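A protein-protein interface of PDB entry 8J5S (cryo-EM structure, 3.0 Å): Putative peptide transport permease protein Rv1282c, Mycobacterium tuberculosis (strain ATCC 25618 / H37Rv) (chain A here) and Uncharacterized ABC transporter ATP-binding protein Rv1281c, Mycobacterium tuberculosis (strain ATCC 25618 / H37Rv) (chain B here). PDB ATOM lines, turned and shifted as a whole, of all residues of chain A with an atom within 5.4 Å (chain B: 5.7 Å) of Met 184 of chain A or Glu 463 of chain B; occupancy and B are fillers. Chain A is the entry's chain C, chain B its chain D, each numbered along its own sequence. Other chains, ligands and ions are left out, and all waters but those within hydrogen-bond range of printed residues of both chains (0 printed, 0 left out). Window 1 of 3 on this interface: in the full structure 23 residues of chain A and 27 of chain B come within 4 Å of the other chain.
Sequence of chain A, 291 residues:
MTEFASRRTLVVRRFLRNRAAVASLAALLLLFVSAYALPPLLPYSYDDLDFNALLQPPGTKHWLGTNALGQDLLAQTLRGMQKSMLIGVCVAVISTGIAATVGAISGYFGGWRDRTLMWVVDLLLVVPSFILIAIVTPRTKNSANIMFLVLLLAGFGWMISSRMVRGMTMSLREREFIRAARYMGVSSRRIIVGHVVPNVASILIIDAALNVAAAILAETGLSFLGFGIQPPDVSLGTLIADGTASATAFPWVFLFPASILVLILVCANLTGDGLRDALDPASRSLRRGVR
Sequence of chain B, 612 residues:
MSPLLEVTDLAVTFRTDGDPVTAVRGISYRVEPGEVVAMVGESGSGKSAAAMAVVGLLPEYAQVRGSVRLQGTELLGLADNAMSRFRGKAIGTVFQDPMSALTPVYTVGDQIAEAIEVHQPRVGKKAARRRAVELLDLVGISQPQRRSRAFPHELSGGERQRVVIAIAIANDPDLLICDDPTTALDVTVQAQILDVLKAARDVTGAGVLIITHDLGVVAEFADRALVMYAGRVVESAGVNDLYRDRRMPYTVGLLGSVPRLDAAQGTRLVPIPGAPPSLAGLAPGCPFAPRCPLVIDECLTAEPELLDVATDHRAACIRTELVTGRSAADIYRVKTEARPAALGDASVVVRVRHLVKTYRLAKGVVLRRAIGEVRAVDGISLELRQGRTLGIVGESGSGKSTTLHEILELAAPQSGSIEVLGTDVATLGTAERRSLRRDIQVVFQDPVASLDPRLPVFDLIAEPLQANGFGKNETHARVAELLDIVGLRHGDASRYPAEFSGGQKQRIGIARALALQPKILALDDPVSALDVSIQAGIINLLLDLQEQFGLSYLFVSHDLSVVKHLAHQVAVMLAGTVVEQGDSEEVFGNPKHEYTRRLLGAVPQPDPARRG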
ATOM      1  N   ARG A 179     -35.907   3.877 -36.993  1.00  0.00           N
ATOM      2  CA  ARG A 179     -36.924   4.456 -36.125  1.00  0.00           C
ATOM      3  C   ARG A 179     -36.588   4.234 -34.662  1.00  0.00           C
ATOM      4  O   ARG A 179     -36.749   5.139 -33.836  1.00  0.00           O
ATOM      5  CB  ARG A 179     -38.285   3.859 -36.447  1.00  0.00           C
ATOM      6  CG  ARG A 179     -39.407   4.471 -35.662  1.00  0.00           C
ATOM      7  CD  ARG A 179     -40.684   4.405 -36.446  1.00  0.00           C
ATOM      8  NE  ARG A 179     -41.298   3.092 -36.350  1.00  0.00           N
ATOM      9  CZ  ARG A 179     -42.425   2.858 -35.696  1.00  0.00           C
ATOM     10  NH1 ARG A 179     -43.052   3.852 -35.090  1.00  0.00           N
ATOM     11  NH2 ARG A 179     -42.928   1.635 -35.652  1.00  0.00           N
ATOM     12  N   ALA A 180     -36.117   3.036 -34.318  1.00  0.00           N
ATOM     13  CA  ALA A 180     -35.650   2.802 -32.957  1.00  0.00           C
ATOM     14  C   ALA A 180     -34.485   3.718 -32.613  1.00  0.00           C
ATOM     15  O   ALA A 180     -34.387   4.218 -31.486  1.00  0.00           O
ATOM     16  CB  ALA A 180     -35.252   1.344 -32.781  1.00  0.00           C
ATOM     17  N   ALA A 181     -33.595   3.953 -33.577  1.00  0.00           N
ATOM     18  CA  ALA A 181     -32.478   4.863 -33.358  1.00  0.00           C
ATOM     19  C   ALA A 181     -32.968   6.259 -33.022  1.00  0.00           C
ATOM     20  O   ALA A 181     -32.408   6.930 -32.153  1.00  0.00           O
ATOM     21  CB  ALA A 181     -31.581   4.896 -34.589  1.00  0.00           C
ATOM     22  N   ARG A 182     -34.002   6.722 -33.712  1.00  0.00           N
ATOM     23  CA  ARG A 182     -34.590   8.002 -33.340  1.00  0.00           C
ATOM     24  C   ARG A 182     -35.242   7.937 -31.970  1.00  0.00           C
ATOM     25  O   ARG A 182     -35.237   8.930 -31.239  1.00  0.00           O
ATOM     26  CB  ARG A 182     -35.609   8.446 -34.380  1.00  0.00           C
ATOM     27  CG  ARG A 182     -36.189   9.812 -34.106  1.00  0.00           C
ATOM     28  CD  ARG A 182     -37.018  10.287 -35.274  1.00  0.00           C
ATOM     29  NE  ARG A 182     -37.987   9.282 -35.689  1.00  0.00           N
ATOM     30  CZ  ARG A 182     -39.222   9.201 -35.212  1.00  0.00           C
ATOM     31  NH1 ARG A 182     -39.641  10.066 -34.303  1.00  0.00           N
ATOM     32  NH2 ARG A 182     -40.039   8.258 -35.647  1.00  0.00           N
ATOM     33  N   TYR A 183     -35.820   6.790 -31.613  1.00  0.00           N
ATOM     34  CA  TYR A 183     -36.428   6.654 -30.293  1.00  0.00           C
ATOM     35  C   TYR A 183     -35.392   6.740 -29.185  1.00  0.00           C
ATOM     36  O   TYR A 183     -35.725   7.122 -28.063  1.00  0.00           O
ATOM     37  CB  TYR A 183     -37.190   5.336 -30.186  1.00  0.00           C
ATOM     38  CG  TYR A 183     -38.529   5.323 -30.891  1.00  0.00           C
ATOM     39  CD1 TYR A 183     -38.955   4.212 -31.588  1.00  0.00           C
ATOM     40  CD2 TYR A 183     -39.361   6.421 -30.855  1.00  0.00           C
ATOM     41  CE1 TYR A 183     -40.166   4.201 -32.227  1.00  0.00           C
ATOM     42  CE2 TYR A 183     -40.568   6.414 -31.487  1.00  0.00           C
ATOM     43  CZ  TYR A 183     -40.968   5.304 -32.174  1.00  0.00           C
ATOM     44  OH  TYR A 183     -42.184   5.296 -32.817  1.00  0.00           O
ATOM     45  N   MET A 184     -34.140   6.380 -29.471  1.00  0.00           N
ATOM     46  CA  MET A 184     -33.097   6.448 -28.451  1.00  0.00           C
ATOM     47  C   MET A 184     -32.606   7.870 -28.215  1.00  0.00           C
ATOM     48  O   MET A 184     -32.340   8.250 -27.072  1.00  0.00           O
ATOM     49  CB  MET A 184     -31.922   5.563 -28.839  1.00  0.00           C
ATOM     50  CG  MET A 184     -32.283   4.133 -29.024  1.00  0.00           C
ATOM     51  SD  MET A 184     -31.136   3.316 -30.113  1.00  0.00           S
ATOM     52  CE  MET A 184     -31.612   1.635 -29.818  1.00  0.00           C
ATOM     53  N   GLY A 185     -32.462   8.661 -29.269  1.00  0.00           N
ATOM     54  CA  GLY A 185     -31.910   9.990 -29.125  1.00  0.00           C
ATOM     55  C   GLY A 185     -30.785  10.268 -30.098  1.00  0.00           C
ATOM     56  O   GLY A 185     -30.042  11.240 -29.944  1.00  0.00           O
ATOM     57  N   VAL A 186     -30.640   9.409 -31.102  1.00  0.00           N
ATOM     58  CA  VAL A 186     -29.621   9.614 -32.119  1.00  0.00           C
ATOM     59  C   VAL A 186     -30.067  10.718 -33.070  1.00  0.00           C
ATOM     60  O   VAL A 186     -31.233  10.783 -33.476  1.00  0.00           O
ATOM     61  CB  VAL A 186     -29.351   8.296 -32.860  1.00  0.00           C
ATOM     62  CG1 VAL A 186     -28.219   8.460 -33.831  1.00  0.00           C
ATOM     63  CG2 VAL A 186     -29.030   7.199 -31.878  1.00  0.00           C
ATOM     64  N   HIS A 195     -25.747   4.168 -39.810  1.00  0.00           N
ATOM     65  CA  HIS A 195     -26.604   3.135 -40.372  1.00  0.00           C
ATOM     66  C   HIS A 195     -26.611   3.096 -41.890  1.00  0.00           C
ATOM     67  O   HIS A 195     -26.615   2.010 -42.468  1.00  0.00           O
ATOM     68  CB  HIS A 195     -28.039   3.322 -39.869  1.00  0.00           C
ATOM     69  CG  HIS A 195     -28.260   2.845 -38.468  1.00  0.00           C
ATOM     70  ND1 HIS A 195     -28.713   1.579 -38.177  1.00  0.00           N
ATOM     71  CD2 HIS A 195     -28.093   3.467 -37.279  1.00  0.00           C
ATOM     72  CE1 HIS A 195     -28.811   1.440 -36.868  1.00  0.00           C
ATOM     73  NE2 HIS A 195     -28.440   2.570 -36.300  1.00  0.00           N
ATOM     74  N   ARG B 437     -35.959  11.950 -23.850  1.00  0.00           N
ATOM     75  CA  ARG B 437     -35.844  10.640 -24.471  1.00  0.00           C
ATOM     76  C   ARG B 437     -34.816   9.719 -23.827  1.00  0.00           C
ATOM     77  O   ARG B 437     -34.582   8.633 -24.355  1.00  0.00           O
ATOM     78  CB  ARG B 437     -35.516  10.796 -25.948  1.00  0.00           C
ATOM     79  CG  ARG B 437     -36.725  10.735 -26.823  1.00  0.00           C
ATOM     80  CD  ARG B 437     -36.351  10.388 -28.219  1.00  0.00           C
ATOM     81  NE  ARG B 437     -37.268  10.987 -29.171  1.00  0.00           N
ATOM     82  CZ  ARG B 437     -38.468  10.500 -29.457  1.00  0.00           C
ATOM     83  NH1 ARG B 437     -38.902   9.400 -28.865  1.00  0.00           N
ATOM     84  NH2 ARG B 437     -39.232  11.117 -30.343  1.00  0.00           N
ATOM     85  N   ARG B 438     -34.187  10.109 -22.724  1.00  0.00           N
ATOM     86  CA  ARG B 438     -33.267   9.214 -22.032  1.00  0.00           C
ATOM     87  C   ARG B 438     -33.880   8.593 -20.790  1.00  0.00           C
ATOM     88  O   ARG B 438     -33.188   7.873 -20.066  1.00  0.00           O
ATOM     89  CB  ARG B 438     -31.970   9.938 -21.659  1.00  0.00           C
ATOM     90  CG  ARG B 438     -32.147  11.062 -20.680  1.00  0.00           C
ATOM     91  CD  ARG B 438     -30.908  11.255 -19.841  1.00  0.00           C
ATOM     92  NE  ARG B 438     -30.565  10.058 -19.081  1.00  0.00           N
ATOM     93  CZ  ARG B 438     -29.324   9.622 -18.891  1.00  0.00           C
ATOM     94  NH1 ARG B 438     -28.296  10.284 -19.406  1.00  0.00           N
ATOM     95  NH2 ARG B 438     -29.107   8.521 -18.185  1.00  0.00           N
ATOM     96  N   GLN B 441     -38.101   4.514 -22.792  1.00  0.00           N
ATOM     97  CA  GLN B 441     -37.589   3.686 -23.877  1.00  0.00           C
ATOM     98  C   GLN B 441     -38.571   2.593 -24.260  1.00  0.00           C
ATOM     99  O   GLN B 441     -39.699   2.583 -23.770  1.00  0.00           O
ATOM    100  CB  GLN B 441     -36.249   3.085 -23.489  1.00  0.00           C
ATOM    101  CG  GLN B 441     -35.218   4.121 -23.118  1.00  0.00           C
ATOM    102  CD  GLN B 441     -34.640   4.821 -24.315  1.00  0.00           C
ATOM    103  OE1 GLN B 441     -34.861   4.418 -25.447  1.00  0.00           O
ATOM    104  NE2 GLN B 441     -33.882   5.874 -24.069  1.00  0.00           N
ATOM    105  N   LEU B 455     -24.573  -4.804 -37.583  1.00  0.00           N
ATOM    106  CA  LEU B 455     -23.786  -4.341 -36.457  1.00  0.00           C
ATOM    107  C   LEU B 455     -23.629  -5.481 -35.464  1.00  0.00           C
ATOM    108  O   LEU B 455     -24.591  -6.204 -35.201  1.00  0.00           O
ATOM    109  CB  LEU B 455     -24.445  -3.146 -35.760  1.00  0.00           C
ATOM    110  CG  LEU B 455     -24.527  -1.801 -36.466  1.00  0.00           C
ATOM    111  CD1 LEU B 455     -25.705  -1.041 -35.940  1.00  0.00           C
ATOM    112  CD2 LEU B 455     -23.264  -1.016 -36.235  1.00  0.00           C
ATOM    113  N   PHE B 458     -22.202  -5.839 -29.562  1.00  0.00           N
ATOM    114  CA  PHE B 458     -21.676  -4.741 -28.759  1.00  0.00           C
ATOM    115  C   PHE B 458     -22.107  -3.394 -29.314  1.00  0.00           C
ATOM    116  O   PHE B 458     -22.434  -2.480 -28.553  1.00  0.00           O
ATOM    117  CB  PHE B 458     -20.157  -4.814 -28.689  1.00  0.00           C
ATOM    118  CG  PHE B 458     -19.517  -3.544 -28.229  1.00  0.00           C
ATOM    119  CD1 PHE B 458     -18.791  -2.770 -29.104  1.00  0.00           C
ATOM    120  CD2 PHE B 458     -19.640  -3.124 -26.924  1.00  0.00           C
ATOM    121  CE1 PHE B 458     -18.205  -1.605 -28.682  1.00  0.00           C
ATOM    122  CE2 PHE B 458     -19.054  -1.965 -26.499  1.00  0.00           C
ATOM    123  CZ  PHE B 458     -18.338  -1.203 -27.375  1.00  0.00           C
ATOM    124  N   ASP B 459     -22.100  -3.243 -30.634  1.00  0.00           N
ATOM    125  CA  ASP B 459     -22.526  -1.984 -31.226  1.00  0.00           C
ATOM    126  C   ASP B 459     -24.022  -1.772 -31.066  1.00  0.00           C
ATOM    127  O   ASP B 459     -24.472  -0.640 -30.867  1.00  0.00           O
ATOM    128  CB  ASP B 459     -22.129  -1.939 -32.697  1.00  0.00           C
ATOM    129  CG  ASP B 459     -20.657  -1.643 -32.890  1.00  0.00           C
ATOM    130  OD1 ASP B 459     -20.303  -0.455 -33.034  1.00  0.00           O
ATOM    131  OD2 ASP B 459     -19.850  -2.593 -32.880  1.00  0.00           O
ATOM    132  N   LEU B 460     -24.813  -2.840 -31.159  1.00  0.00           N
ATOM    133  CA  LEU B 460     -26.255  -2.705 -31.005  1.00  0.00           C
ATOM    134  C   LEU B 460     -26.620  -2.296 -29.587  1.00  0.00           C
ATOM    135  O   LEU B 460     -27.374  -1.342 -29.381  1.00  0.00           O
ATOM    136  CB  LEU B 460     -26.948  -4.014 -31.368  1.00  0.00           C
ATOM    137  CG  LEU B 460     -26.927  -4.448 -32.823  1.00  0.00           C
ATOM    138  CD1 LEU B 460     -27.506  -5.824 -32.933  1.00  0.00           C
ATOM    139  CD2 LEU B 460     -27.709  -3.478 -33.657  1.00  0.00           C
ATOM    140  N   ILE B 461     -26.092  -3.010 -28.596  1.00  0.00           N
ATOM    141  CA  ILE B 461     -26.445  -2.743 -27.208  1.00  0.00           C
ATOM    142  C   ILE B 461     -25.942  -1.381 -26.773  1.00  0.00           C
ATOM    143  O   ILE B 461     -26.546  -0.734 -25.913  1.00  0.00           O
ATOM    144  CB  ILE B 461     -25.904  -3.858 -26.300  1.00  0.00           C
ATOM    145  CG1 ILE B 461     -26.535  -5.196 -26.671  1.00  0.00           C
ATOM    146  CG2 ILE B 461     -26.174  -3.554 -24.854  1.00  0.00           C
ATOM    147  CD1 ILE B 461     -26.133  -6.322 -25.759  1.00  0.00           C
ATOM    148  N   ALA B 462     -24.849  -0.907 -27.361  1.00  0.00           N
ATOM    149  CA  ALA B 462     -24.196   0.315 -26.917  1.00  0.00           C
ATOM    150  C   ALA B 462     -24.427   1.484 -27.863  1.00  0.00           C
ATOM    151  O   ALA B 462     -23.619   2.406 -27.911  1.00  0.00           O
ATOM    152  CB  ALA B 462     -22.702   0.085 -26.730  1.00  0.00           C
ATOM    153  N   GLU B 463     -25.505   1.456 -28.636  1.00  0.00           N
ATOM    154  CA  GLU B 463     -25.918   2.657 -29.352  1.00  0.00           C
ATOM    155  C   GLU B 463     -26.698   3.607 -28.451  1.00  0.00           C
ATOM    156  O   GLU B 463     -26.479   4.817 -28.527  1.00  0.00           O
ATOM    157  CB  GLU B 463     -26.740   2.325 -30.592  1.00  0.00           C
ATOM    158  CG  GLU B 463     -26.739   3.451 -31.601  1.00  0.00           C
ATOM    159  CD  GLU B 463     -27.656   3.202 -32.779  1.00  0.00           C
ATOM    160  OE1 GLU B 463     -28.673   2.501 -32.600  1.00  0.00           O
ATOM    161  OE2 GLU B 463     -27.361   3.710 -33.885  1.00  0.00           O
ATOM    162  N   PRO B 464     -27.617   3.136 -27.600  1.00  0.00           N
ATOM    163  CA  PRO B 464     -28.287   4.064 -26.680  1.00  0.00           C
ATOM    164  C   PRO B 464     -27.360   4.720 -25.684  1.00  0.00           C
ATOM    165  O   PRO B 464     -27.809   5.602 -24.946  1.00  0.00           O
ATOM    166  CB  PRO B 464     -29.314   3.175 -25.971  1.00  0.00           C
ATOM    167  CG  PRO B 464     -28.801   1.810 -26.133  1.00  0.00           C
ATOM    168  CD  PRO B 464     -28.203   1.791 -27.487  1.00  0.00           C
ATOM    169  N   LEU B 465     -26.094   4.323 -25.624  1.00  0.00           N
ATOM    170  CA  LEU B 465     -25.139   4.899 -24.691  1.00  0.00           C
ATOM    171  C   LEU B 465     -24.168   5.852 -25.360  1.00  0.00           C
ATOM    172  O   LEU B 465     -23.878   6.912 -24.813  1.00  0.00           O
ATOM    173  CB  LEU B 465     -24.358   3.790 -23.985  1.00  0.00           C
ATOM    174  CG  LEU B 465     -25.126   2.911 -23.004  1.00  0.00           C
ATOM    175  CD1 LEU B 465     -24.348   1.660 -22.728  1.00  0.00           C
ATOM    176  CD2 LEU B 465     -25.394   3.650 -21.721  1.00  0.00           C
ATOM    177  N   GLN B 466     -23.651   5.498 -26.534  1.00  0.00           N
ATOM    178  CA  GLN B 466     -22.784   6.420 -27.252  1.00  0.00           C
ATOM    179  C   GLN B 466     -23.528   7.685 -27.625  1.00  0.00           C
ATOM    180  O   GLN B 466     -22.970   8.784 -27.564  1.00  0.00           O
ATOM    181  CB  GLN B 466     -22.224   5.756 -28.506  1.00  0.00           C
ATOM    182  CG  GLN B 466     -21.464   4.483 -28.263  1.00  0.00           C
ATOM    183  CD  GLN B 466     -21.288   3.691 -29.530  1.00  0.00           C
ATOM    184  OE1 GLN B 466     -21.894   4.003 -30.553  1.00  0.00           O
ATOM    185  NE2 GLN B 466     -20.464   2.653 -29.474  1.00  0.00           N
ATOM    186  N   ALA B 467     -24.789   7.545 -28.034  1.00  0.00           N
ATOM    187  CA  ALA B 467     -25.579   8.703 -28.429  1.00  0.00           C
ATOM    188  C   ALA B 467     -25.810   9.646 -27.259  1.00  0.00           C
ATOM    189  O   ALA B 467     -25.689  10.865 -27.403  1.00  0.00           O
ATOM    190  CB  ALA B 467     -26.908   8.242 -29.018  1.00  0.00           C
ATOM    191  N   ASN B 468     -26.130   9.108 -26.095  1.00  0.00           N
ATOM    192  CA  ASN B 468     -26.479   9.928 -24.946  1.00  0.00           C
ATOM    193  C   ASN B 468     -25.210  10.394 -24.243  1.00  0.00           C
ATOM    194  O   ASN B 468     -24.108  10.330 -24.789  1.00  0.00           O
ATOM    195  CB  ASN B 468     -27.414   9.166 -24.017  1.00  0.00           C
ATOM    196  CG  ASN B 468     -28.870   9.499 -24.265  1.00  0.00           C
ATOM    197  OD1 ASN B 468     -29.434  10.380 -23.621  1.00  0.00           O
ATOM    198  ND2 ASN B 468     -29.484   8.802 -25.208  1.00  0.00           N
ATOM    199  N   ARG B 512     -30.678  -3.832 -24.692  1.00  0.00           N
ATOM    200  CA  ARG B 512     -30.464  -2.534 -25.315  1.00  0.00           C
ATOM    201  C   ARG B 512     -31.401  -1.485 -24.745  1.00  0.00           C
ATOM    202  O   ARG B 512     -30.998  -0.339 -24.530  1.00  0.00           O
ATOM    203  CB  ARG B 512     -30.646  -2.663 -26.821  1.00  0.00           C
ATOM    204  CG  ARG B 512     -30.828  -1.380 -27.549  1.00  0.00           C
ATOM    205  CD  ARG B 512     -30.773  -1.632 -29.033  1.00  0.00           C
ATOM    206  NE  ARG B 512     -32.105  -1.675 -29.621  1.00  0.00           N
ATOM    207  CZ  ARG B 512     -32.339  -1.893 -30.907  1.00  0.00           C
ATOM    208  NH1 ARG B 512     -31.330  -2.079 -31.738  1.00  0.00           N
ATOM    209  NH2 ARG B 512     -33.578  -1.919 -31.362  1.00  0.00           N
ATOM    210  N   LEU B 516     -29.810   2.666 -20.541  1.00  0.00           N
ATOM    211  CA  LEU B 516     -29.773   3.964 -19.885  1.00  0.00           C
ATOM    212  C   LEU B 516     -30.449   3.967 -18.528  1.00  0.00           C
ATOM    213  O   LEU B 516     -30.427   5.000 -17.854  1.00  0.00           O
ATOM    214  CB  LEU B 516     -30.419   5.017 -20.779  1.00  0.00           C
ATOM    215  CG  LEU B 516     -29.630   5.339 -22.037  1.00  0.00           C
ATOM    216  CD1 LEU B 516     -30.426   6.253 -22.928  1.00  0.00           C
ATOM    217  CD2 LEU B 516     -28.331   5.983 -21.644  1.00  0.00           C
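The guanidinium group (NH1) of Arg 179 of chain A lies within hydrogen-bond range of the side-chain hydroxyl (OH) of Tyr 183 of chain A (2.8 Å). The backbone NH (N) of Val 186 of chain A is in hydrogen-bond range of the backbone carbonyl oxygen (O) of Ala 181 of chain A (3.2 Å). The backbone carbonyl oxygen (O) of Arg 437 of chain B is in hydrogen-bond range of the side-chain amide nitrogen (NE2) of Gln 441 of chain B.
The backbone carbonyl oxygen of Met 184 of chain A sits at hydrogen-bond distance from the side-chain amide nitrogen of Asn 468 of chain B (3.5 Å). NE2 of His 195 of chain A is in hydrogen-bond range of OE2 of Glu 463 of chain B (2.9 Å). The side-chain sulfur of Met 184 of chain A sits close to the side-chain carboxylate of Glu 463 of chain B (3.6 Å).
Ala 180 of chain A touches Arg 512 of chain B. Arg 182 of chain A touches Arg 437 of chain B (O to CD, 3.5 Å). O of Tyr 183 of chain A touches CD of Arg 437 of chain B (3.3 Å). OE1 of Gln 441 of chain B touches O of Tyr 183 of chain A (3.9 Å). Met 184 of chain A touches Arg 437 of chain B. Arg 512 of chain B touches Met 184 of chain A. CB of Ala 467 of chain B touches CG2 of Val 186 of chain A, 3.7 Å away.
Met 184 of chain A touches just these residues of chain B: Arg 437 (3.5 Å), Glu 463 (3.6 Å), Asn 468 (3.5 Å) and Arg 512 (3.4 Å). Of the printed residues of chain A, Gln 441 of chain B touches Tyr 183. Printed residues of chain B within 4 Å of Val 186 of chain A: Ala 467.
Hydrophobic or aromatic side chains of chain A that line the printed part of chain B: Ala 180, Tyr 183, Met 184, Val 186 and His 195. Printed residues of chain B that touch a printed residue of chain A: Arg 437, Gln 441, Glu 463, Ala 467, Asn 468 and Arg 512. Among the printed residues, 10 pairs touch across the chains. Among the printed residues, no Asp or Glu carboxylate lies within 4 Å of a Lys or Arg side-chain nitrogen of the other chain.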
